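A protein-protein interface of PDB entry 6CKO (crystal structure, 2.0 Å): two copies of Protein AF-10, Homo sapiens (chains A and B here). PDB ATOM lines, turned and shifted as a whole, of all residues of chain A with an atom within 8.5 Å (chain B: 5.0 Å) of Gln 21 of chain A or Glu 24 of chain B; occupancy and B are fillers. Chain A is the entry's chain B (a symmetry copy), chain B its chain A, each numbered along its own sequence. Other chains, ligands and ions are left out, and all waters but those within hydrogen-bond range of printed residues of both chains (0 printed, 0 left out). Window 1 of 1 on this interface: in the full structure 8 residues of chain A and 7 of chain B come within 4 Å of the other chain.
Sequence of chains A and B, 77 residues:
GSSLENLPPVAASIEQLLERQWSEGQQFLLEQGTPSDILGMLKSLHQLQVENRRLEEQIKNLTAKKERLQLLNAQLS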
ATOM      1  N   ILE A  14      15.592 -16.121  -7.702  1.00  0.00           N
ATOM      2  CA  ILE A  14      16.438 -16.277  -6.523  1.00  0.00           C
ATOM      3  C   ILE A  14      16.704 -14.911  -5.912  1.00  0.00           C
ATOM      4  O   ILE A  14      16.630 -14.770  -4.705  1.00  0.00           O
ATOM      5  CB  ILE A  14      17.800 -16.952  -6.797  1.00  0.00           C
ATOM      6  CG1 ILE A  14      17.631 -18.177  -7.700  1.00  0.00           C
ATOM      7  CG2 ILE A  14      18.462 -17.361  -5.474  1.00  0.00           C
ATOM      8  N   GLU A  15      16.998 -13.910  -6.743  1.00  0.00           N
ATOM      9  CA  GLU A  15      17.245 -12.547  -6.240  1.00  0.00           C
ATOM     10  C   GLU A  15      16.070 -12.035  -5.368  1.00  0.00           C
ATOM     11  O   GLU A  15      16.297 -11.500  -4.288  1.00  0.00           O
ATOM     12  CB  GLU A  15      17.538 -11.548  -7.366  1.00  0.00           C
ATOM     13  CG  GLU A  15      18.871 -11.771  -8.095  1.00  0.00           C
ATOM     14  CD  GLU A  15      18.808 -12.795  -9.228  1.00  0.00           C
ATOM     15  OE1 GLU A  15      19.870 -13.107  -9.819  1.00  0.00           O
ATOM     16  OE2 GLU A  15      17.695 -13.291  -9.537  1.00  0.00           O
ATOM     17  N   GLN A  16      14.835 -12.232  -5.830  1.00  0.00           N
ATOM     18  CA  GLN A  16      13.665 -11.765  -5.110  1.00  0.00           C
ATOM     19  C   GLN A  16      13.482 -12.570  -3.817  1.00  0.00           C
ATOM     20  O   GLN A  16      13.173 -11.994  -2.783  1.00  0.00           O
ATOM     21  CB  GLN A  16      12.405 -11.836  -5.980  1.00  0.00           C
ATOM     22  CG  GLN A  16      12.472 -11.060  -7.300  1.00  0.00           C
ATOM     23  N   LEU A  17      13.702 -13.882  -3.874  1.00  0.00           N
ATOM     24  CA  LEU A  17      13.667 -14.715  -2.674  1.00  0.00           C
ATOM     25  C   LEU A  17      14.689 -14.289  -1.608  1.00  0.00           C
ATOM     26  O   LEU A  17      14.362 -14.224  -0.424  1.00  0.00           O
ATOM     27  CB  LEU A  17      13.868 -16.191  -3.027  1.00  0.00           C
ATOM     28  CG  LEU A  17      13.833 -17.167  -1.837  1.00  0.00           C
ATOM     29  CD1 LEU A  17      12.544 -17.058  -1.017  1.00  0.00           C
ATOM     30  CD2 LEU A  17      14.029 -18.588  -2.326  1.00  0.00           C
ATOM     31  N   LEU A  18      15.917 -14.023  -2.034  1.00  0.00           N
ATOM     32  CA  LEU A  18      16.983 -13.593  -1.119  1.00  0.00           C
ATOM     33  C   LEU A  18      16.660 -12.241  -0.504  1.00  0.00           C
ATOM     34  O   LEU A  18      16.918 -12.005   0.678  1.00  0.00           O
ATOM     35  CB  LEU A  18      18.332 -13.498  -1.836  1.00  0.00           C
ATOM     36  CG  LEU A  18      18.951 -14.803  -2.342  1.00  0.00           C
ATOM     37  CD1 LEU A  18      20.298 -14.523  -3.040  1.00  0.00           C
ATOM     38  CD2 LEU A  18      19.112 -15.806  -1.210  1.00  0.00           C
ATOM     39  N   GLU A  19      16.116 -11.356  -1.328  1.00  0.00           N
ATOM     40  CA  GLU A  19      15.696 -10.052  -0.869  1.00  0.00           C
ATOM     41  C   GLU A  19      14.558 -10.155   0.172  1.00  0.00           C
ATOM     42  O   GLU A  19      14.585  -9.452   1.175  1.00  0.00           O
ATOM     43  CB  GLU A  19      15.275  -9.197  -2.057  1.00  0.00           C
ATOM     44  CG  GLU A  19      15.272  -7.722  -1.776  1.00  0.00           C
ATOM     45  CD  GLU A  19      16.633  -7.141  -1.452  1.00  0.00           C
ATOM     46  OE1 GLU A  19      16.618  -6.026  -0.946  1.00  0.00           O
ATOM     47  OE2 GLU A  19      17.681  -7.755  -1.697  1.00  0.00           O
ATOM     48  N   ARG A  20      13.604 -11.050  -0.062  1.00  0.00           N
ATOM     49  CA  ARG A  20      12.544 -11.331   0.909  1.00  0.00           C
ATOM     50  C   ARG A  20      13.092 -11.933   2.208  1.00  0.00           C
ATOM     51  O   ARG A  20      12.728 -11.504   3.305  1.00  0.00           O
ATOM     52  CB  ARG A  20      11.485 -12.271   0.323  1.00  0.00           C
ATOM     53  CG  ARG A  20      10.447 -12.652   1.367  1.00  0.00           C
ATOM     54  CD  ARG A  20       9.118 -13.155   0.822  1.00  0.00           C
ATOM     55  NE  ARG A  20       9.135 -14.462   0.160  1.00  0.00           N
ATOM     56  CZ  ARG A  20       9.509 -15.625   0.705  1.00  0.00           C
ATOM     57  NH1 ARG A  20       9.425 -16.737  -0.030  1.00  0.00           N
ATOM     58  NH2 ARG A  20       9.991 -15.712   1.949  1.00  0.00           N
ATOM     59  N   GLN A  21      13.950 -12.947   2.074  1.00  0.00           N
ATOM     60  CA  GLN A  21      14.553 -13.606   3.219  1.00  0.00           C
ATOM     61  C   GLN A  21      15.408 -12.681   4.092  1.00  0.00           C
ATOM     62  O   GLN A  21      15.371 -12.778   5.323  1.00  0.00           O
ATOM     63  CB  GLN A  21      15.348 -14.818   2.769  1.00  0.00           C
ATOM     64  CG  GLN A  21      14.426 -15.979   2.405  1.00  0.00           C
ATOM     65  CD  GLN A  21      15.170 -17.258   2.230  1.00  0.00           C
ATOM     66  OE1 GLN A  21      16.377 -17.246   2.126  1.00  0.00           O
ATOM     67  NE2 GLN A  21      14.460 -18.373   2.207  1.00  0.00           N
ATOM     68  N   TRP A  22      16.154 -11.797   3.447  1.00  0.00           N
ATOM     69  CA  TRP A  22      16.840 -10.705   4.124  1.00  0.00           C
ATOM     70  C   TRP A  22      15.881  -9.763   4.904  1.00  0.00           C
ATOM     71  O   TRP A  22      16.189  -9.397   6.045  1.00  0.00           O
ATOM     72  CB  TRP A  22      17.661  -9.887   3.130  1.00  0.00           C
ATOM     73  CG  TRP A  22      17.951  -8.492   3.572  1.00  0.00           C
ATOM     74  CD1 TRP A  22      17.354  -7.340   3.123  1.00  0.00           C
ATOM     75  CD2 TRP A  22      18.894  -8.098   4.555  1.00  0.00           C
ATOM     76  NE1 TRP A  22      17.876  -6.250   3.776  1.00  0.00           N
ATOM     77  CE2 TRP A  22      18.829  -6.686   4.659  1.00  0.00           C
ATOM     78  CE3 TRP A  22      19.794  -8.803   5.374  1.00  0.00           C
ATOM     79  CZ2 TRP A  22      19.645  -5.960   5.533  1.00  0.00           C
ATOM     80  CZ3 TRP A  22      20.607  -8.081   6.245  1.00  0.00           C
ATOM     81  CH2 TRP A  22      20.520  -6.673   6.321  1.00  0.00           C
ATOM     82  N   SER A  23      14.763  -9.366   4.294  1.00  0.00           N
ATOM     83  CA  SER A  23      13.779  -8.505   4.970  1.00  0.00           C
ATOM     84  C   SER A  23      13.269  -9.128   6.256  1.00  0.00           C
ATOM     85  O   SER A  23      13.254  -8.478   7.295  1.00  0.00           O
ATOM     86  CB  SER A  23      12.572  -8.223   4.090  1.00  0.00           C
ATOM     87  OG  SER A  23      12.932  -7.363   3.049  1.00  0.00           O
ATOM     88  N   GLU A  24      12.836 -10.383   6.150  1.00  0.00           N
ATOM     89  CA  GLU A  24      12.426 -11.212   7.295  1.00  0.00           C
ATOM     90  C   GLU A  24      13.469 -11.226   8.412  1.00  0.00           C
ATOM     91  O   GLU A  24      13.138 -11.123   9.581  1.00  0.00           O
ATOM     92  CB  GLU A  24      12.224 -12.644   6.839  1.00  0.00           C
ATOM     93  CG  GLU A  24      11.031 -12.854   5.926  1.00  0.00           C
ATOM     94  CD  GLU A  24      10.930 -14.284   5.400  1.00  0.00           C
ATOM     95  OE1 GLU A  24      11.825 -15.134   5.710  1.00  0.00           O
ATOM     96  OE2 GLU A  24       9.924 -14.550   4.683  1.00  0.00           O
ATOM     97  N   GLY A  25      14.731 -11.383   8.034  1.00  0.00           N
ATOM     98  CA  GLY A  25      15.833 -11.436   8.979  1.00  0.00           C
ATOM     99  C   GLY A  25      16.100 -10.106   9.648  1.00  0.00           C
ATOM    100  O   GLY A  25      16.307 -10.050  10.857  1.00  0.00           O
ATOM    101  N   GLN A  26      16.133  -9.039   8.860  1.00  0.00           N
ATOM    102  CA  GLN A  26      16.223  -7.688   9.403  1.00  0.00           C
ATOM    103  C   GLN A  26      15.031  -7.422  10.331  1.00  0.00           C
ATOM    104  O   GLN A  26      15.228  -6.927  11.420  1.00  0.00           O
ATOM    105  CB  GLN A  26      16.290  -6.616   8.299  1.00  0.00           C
ATOM    106  CG  GLN A  26      17.225  -5.450   8.620  1.00  0.00           C
ATOM    107  N   GLN A  27      13.820  -7.791   9.929  1.00  0.00           N
ATOM    108  CA  GLN A  27      12.637  -7.573  10.777  1.00  0.00           C
ATOM    109  C   GLN A  27      12.767  -8.344  12.116  1.00  0.00           C
ATOM    110  O   GLN A  27      12.400  -7.822  13.171  1.00  0.00           O
ATOM    111  CB  GLN A  27      11.335  -7.943  10.047  1.00  0.00           C
ATOM    112  CG  GLN A  27      10.081  -7.230  10.570  1.00  0.00           C
ATOM    113  N   PHE A  28      13.339  -9.552  12.068  1.00  0.00           N
ATOM    114  CA  PHE A  28      13.586 -10.349  13.252  1.00  0.00           C
ATOM    115  C   PHE A  28      14.624  -9.737  14.188  1.00  0.00           C
ATOM    116  O   PHE A  28      14.401  -9.644  15.401  1.00  0.00           O
ATOM    117  CB  PHE A  28      14.020 -11.764  12.861  1.00  0.00           C
ATOM    118  CG  PHE A  28      14.316 -12.652  14.031  1.00  0.00           C
ATOM    119  CD1 PHE A  28      15.601 -12.688  14.585  1.00  0.00           C
ATOM    120  CD2 PHE A  28      13.320 -13.444  14.583  1.00  0.00           C
ATOM    121  CE1 PHE A  28      15.883 -13.507  15.672  1.00  0.00           C
ATOM    122  CE2 PHE A  28      13.584 -14.265  15.676  1.00  0.00           C
ATOM    123  CZ  PHE A  28      14.869 -14.295  16.223  1.00  0.00           C
ATOM    124  N   HIS A  46      24.878  -7.427   3.208  1.00  0.00           N
ATOM    125  CA  HIS A  46      23.784  -7.830   2.322  1.00  0.00           C
ATOM    126  C   HIS A  46      23.901  -7.163   0.947  1.00  0.00           C
ATOM    127  O   HIS A  46      23.812  -7.840  -0.058  1.00  0.00           O
ATOM    128  CB  HIS A  46      22.427  -7.511   2.948  1.00  0.00           C
ATOM    129  CG  HIS A  46      21.314  -7.419   1.963  1.00  0.00           C
ATOM    130  ND1 HIS A  46      20.746  -8.527   1.380  1.00  0.00           N
ATOM    131  CD2 HIS A  46      20.675  -6.347   1.444  1.00  0.00           C
ATOM    132  CE1 HIS A  46      19.798  -8.147   0.549  1.00  0.00           C
ATOM    133  NE2 HIS A  46      19.736  -6.827   0.568  1.00  0.00           N
ATOM    134  N   ARG B  20      13.721 -22.308   8.569  1.00  0.00           N
ATOM    135  CA  ARG B  20      12.570 -22.098   7.684  1.00  0.00           C
ATOM    136  C   ARG B  20      13.034 -21.549   6.312  1.00  0.00           C
ATOM    137  O   ARG B  20      12.586 -22.025   5.262  1.00  0.00           O
ATOM    138  CB  ARG B  20      11.584 -21.141   8.332  1.00  0.00           C
ATOM    139  N   GLN B  21      13.958 -20.585   6.347  1.00  0.00           N
ATOM    140  CA  GLN B  21      14.574 -20.008   5.134  1.00  0.00           C
ATOM    141  C   GLN B  21      15.355 -21.001   4.317  1.00  0.00           C
ATOM    142  O   GLN B  21      15.235 -21.024   3.090  1.00  0.00           O
ATOM    143  CB  GLN B  21      15.446 -18.806   5.490  1.00  0.00           C
ATOM    144  CG  GLN B  21      14.563 -17.650   5.926  1.00  0.00           C
ATOM    145  CD  GLN B  21      15.301 -16.380   6.172  1.00  0.00           C
ATOM    146  OE1 GLN B  21      16.509 -16.394   6.380  1.00  0.00           O
ATOM    147  NE2 GLN B  21      14.567 -15.261   6.201  1.00  0.00           N
ATOM    148  N   TRP B  22      16.128 -21.847   4.988  1.00  0.00           N
ATOM    149  CA  TRP B  22      16.762 -22.983   4.317  1.00  0.00           C
ATOM    150  C   TRP B  22      15.705 -23.874   3.643  1.00  0.00           C
ATOM    151  O   TRP B  22      15.847 -24.197   2.473  1.00  0.00           O
ATOM    152  CB  TRP B  22      17.646 -23.797   5.282  1.00  0.00           C
ATOM    153  CG  TRP B  22      18.004 -25.157   4.771  1.00  0.00           C
ATOM    154  CD1 TRP B  22      17.655 -26.349   5.322  1.00  0.00           C
ATOM    155  CD2 TRP B  22      18.742 -25.454   3.599  1.00  0.00           C
ATOM    156  NE1 TRP B  22      18.157 -27.386   4.572  1.00  0.00           N
ATOM    157  CE2 TRP B  22      18.823 -26.864   3.499  1.00  0.00           C
ATOM    158  CE3 TRP B  22      19.335 -24.666   2.606  1.00  0.00           C
ATOM    159  CZ2 TRP B  22      19.466 -27.513   2.440  1.00  0.00           C
ATOM    160  CZ3 TRP B  22      19.993 -25.309   1.542  1.00  0.00           C
ATOM    161  CH2 TRP B  22      20.050 -26.727   1.468  1.00  0.00           C
ATOM    162  N   SER B  23      14.655 -24.256   4.379  1.00  0.00           N
ATOM    163  CA  SER B  23      13.539 -25.049   3.814  1.00  0.00           C
ATOM    164  C   SER B  23      12.895 -24.386   2.567  1.00  0.00           C
ATOM    165  O   SER B  23      12.644 -25.085   1.581  1.00  0.00           O
ATOM    166  CB  SER B  23      12.462 -25.381   4.880  1.00  0.00           C
ATOM    167  N   GLU B  24      12.678 -23.061   2.608  1.00  0.00           N
ATOM    168  CA  GLU B  24      12.161 -22.285   1.470  1.00  0.00           C
ATOM    169  C   GLU B  24      13.106 -22.360   0.266  1.00  0.00           C
ATOM    170  O   GLU B  24      12.681 -22.706  -0.864  1.00  0.00           O
ATOM    171  CB  GLU B  24      12.029 -20.793   1.808  1.00  0.00           C
ATOM    172  CG  GLU B  24      10.865 -20.348   2.657  1.00  0.00           C
ATOM    173  CD  GLU B  24      10.984 -18.880   3.059  1.00  0.00           C
ATOM    174  OE1 GLU B  24      10.706 -18.551   4.251  1.00  0.00           O
ATOM    175  OE2 GLU B  24      11.353 -18.045   2.188  1.00  0.00           O
ATOM    176  N   GLY B  25      14.369 -21.994   0.508  1.00  0.00           N
ATOM    177  CA  GLY B  25      15.356 -21.894  -0.547  1.00  0.00           C
ATOM    178  C   GLY B  25      15.562 -23.204  -1.267  1.00  0.00           C
ATOM    179  O   GLY B  25      15.646 -23.256  -2.494  1.00  0.00           O
ATOM    180  N   GLN B  26      15.651 -24.265  -0.478  1.00  0.00           N
ATOM    181  CA  GLN B  26      15.850 -25.631  -0.961  1.00  0.00           C
ATOM    182  C   GLN B  26      14.682 -26.063  -1.869  1.00  0.00           C
ATOM    183  O   GLN B  26      14.900 -26.647  -2.932  1.00  0.00           O
ATOM    184  CB  GLN B  26      15.982 -26.529   0.273  1.00  0.00           C
ATOM    185  CG  GLN B  26      16.464 -27.954   0.145  1.00  0.00           C
ATOM    186  CD  GLN B  26      16.235 -28.712   1.473  1.00  0.00           C
ATOM    187  OE1 GLN B  26      15.767 -28.135   2.471  1.00  0.00           O
ATOM    188  NE2 GLN B  26      16.552 -29.999   1.485  1.00  0.00           N
ATOM    189  N   GLN B  27      13.452 -25.751  -1.463  1.00  0.00           N
ATOM    190  CA  GLN B  27      12.266 -26.038  -2.290  1.00  0.00           C
ATOM    191  C   GLN B  27      12.317 -25.253  -3.600  1.00  0.00           C
ATOM    192  O   GLN B  27      12.145 -25.820  -4.692  1.00  0.00           O
ATOM    193  CB  GLN B  27      10.955 -25.726  -1.536  1.00  0.00           C
ATOM    194  N   PHE B  28      12.562 -23.951  -3.488  1.00  0.00           N
ATOM    195  CA  PHE B  28      12.634 -23.068  -4.665  1.00  0.00           C
ATOM    196  C   PHE B  28      13.643 -23.586  -5.705  1.00  0.00           C
ATOM    197  O   PHE B  28      13.335 -23.713  -6.901  1.00  0.00           O
ATOM    198  CB  PHE B  28      13.001 -21.650  -4.211  1.00  0.00           C
ATOM    199  CG  PHE B  28      13.096 -20.665  -5.335  1.00  0.00           C
ATOM    200  CD1 PHE B  28      11.946 -20.075  -5.850  1.00  0.00           C
ATOM    201  CD2 PHE B  28      14.321 -20.344  -5.894  1.00  0.00           C
ATOM    202  CE1 PHE B  28      12.011 -19.169  -6.892  1.00  0.00           C
ATOM    203  CE2 PHE B  28      14.399 -19.451  -6.953  1.00  0.00           C
ATOM    204  CZ  PHE B  28      13.240 -18.860  -7.447  1.00  0.00           C
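The side-chain amide nitrogen (NE2) of Gln 21 of chain B is in hydrogen-bond range of the backbone carbonyl oxygen (O) of Gln 21 of chain A, at 2.8 Å.
The side-chain carboxylate (OE1) of Glu 24 of chain A is in hydrogen-bond range of the side-chain amide nitrogen (NE2) of Gln 21 of chain B (2.8 Å).
The side-chain carboxylate (OE2) of Glu 24 of chain B is in salt-bridge range of the guanidinium group (NH2) of Arg 20 of chain A.
OE2 of Glu 24 of chain B is in hydrogen-bond range of NE2 of Gln 21 of chain A (3.1 Å).
The guanidinium group (NH2) of Arg 20 of chain A lies within salt-bridge range of the side-chain carboxylate (OE2) of Glu 24 of chain A, 3.0 Å away.
Among the printed residues, merely in contact across the chains: Ile 14 of chain A with Phe 28 of chain B (3.6 Å), Leu 17 of chain A with Glu 24 of chain B (3.6 Å), Leu 17 of chain A with Gly 25 of chain B (3.98 Å), Leu 17 of chain A with Phe 28 of chain B (3.7 Å) and Glu 24 of chain A with Glu 24 of chain B (3.9 Å).
Of the printed residues of chain B, Gln 21 of chain A touches Gln 21 (2.8 Å) and Glu 24 (3.1 Å).
Of the printed residues of chain B, Glu 24 of chain A touches Gln 21 (2.8 Å) and Glu 24 (3.9 Å).
Printed residues of chain A within 4 Å of Phe 28 of chain B: Ile 14 and Leu 17.
Printed residues of chain B within 4 Å of Leu 17 of chain A: Glu 24, Gly 25 and Phe 28.
Of the printed residues of chain B, Ile 14 of chain A touches Phe 28 (3.6 Å).
Printed residues of chain A within 4 Å of Gly 25 of chain B: Leu 17.
Gln 16 of chain A touches none of the printed residues of chain B.
Trp 22 of chain B touches none of the printed residues of chain A.
The nearest printed residue of chain B that does not touch Ile 14 of chain A is Gly 25 of chain B (7.2 Å).
Printed residues of chain A that touch a printed residue of chain B: Ile 14, Leu 17, Arg 20, Gln 21 and Glu 24.
Hydrophobic or aromatic side chains of chain A that line the printed part of chain B: Ile 14 and Leu 17.
Printed residues of chain B that touch a printed residue of chain A: Gln 21, Glu 24, Gly 25 and Phe 28.
Among the printed residues, Asp or Glu carboxylates within 4 Å of a Lys or Arg side-chain nitrogen of the other chain: Arg 20 of chain A with Glu 24 of chain B (2.7 Å).
Arg 20 of chain A touches Glu 24 of chain B, but with the chains exchanged Glu 24 of chain A does not touch Arg 20 of chain B (6.6 Å).
Gln 21 of chain A touches its own counterpart, Gln 21 of chain B.
Gln 21 of chain A touches Glu 24 of chain B, and with the chains exchanged Glu 24 of chain A touches Gln 21 of chain B.
Glu 24 of chain A touches its own counterpart, Glu 24 of chain B.
9 positions are printed for both chains.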
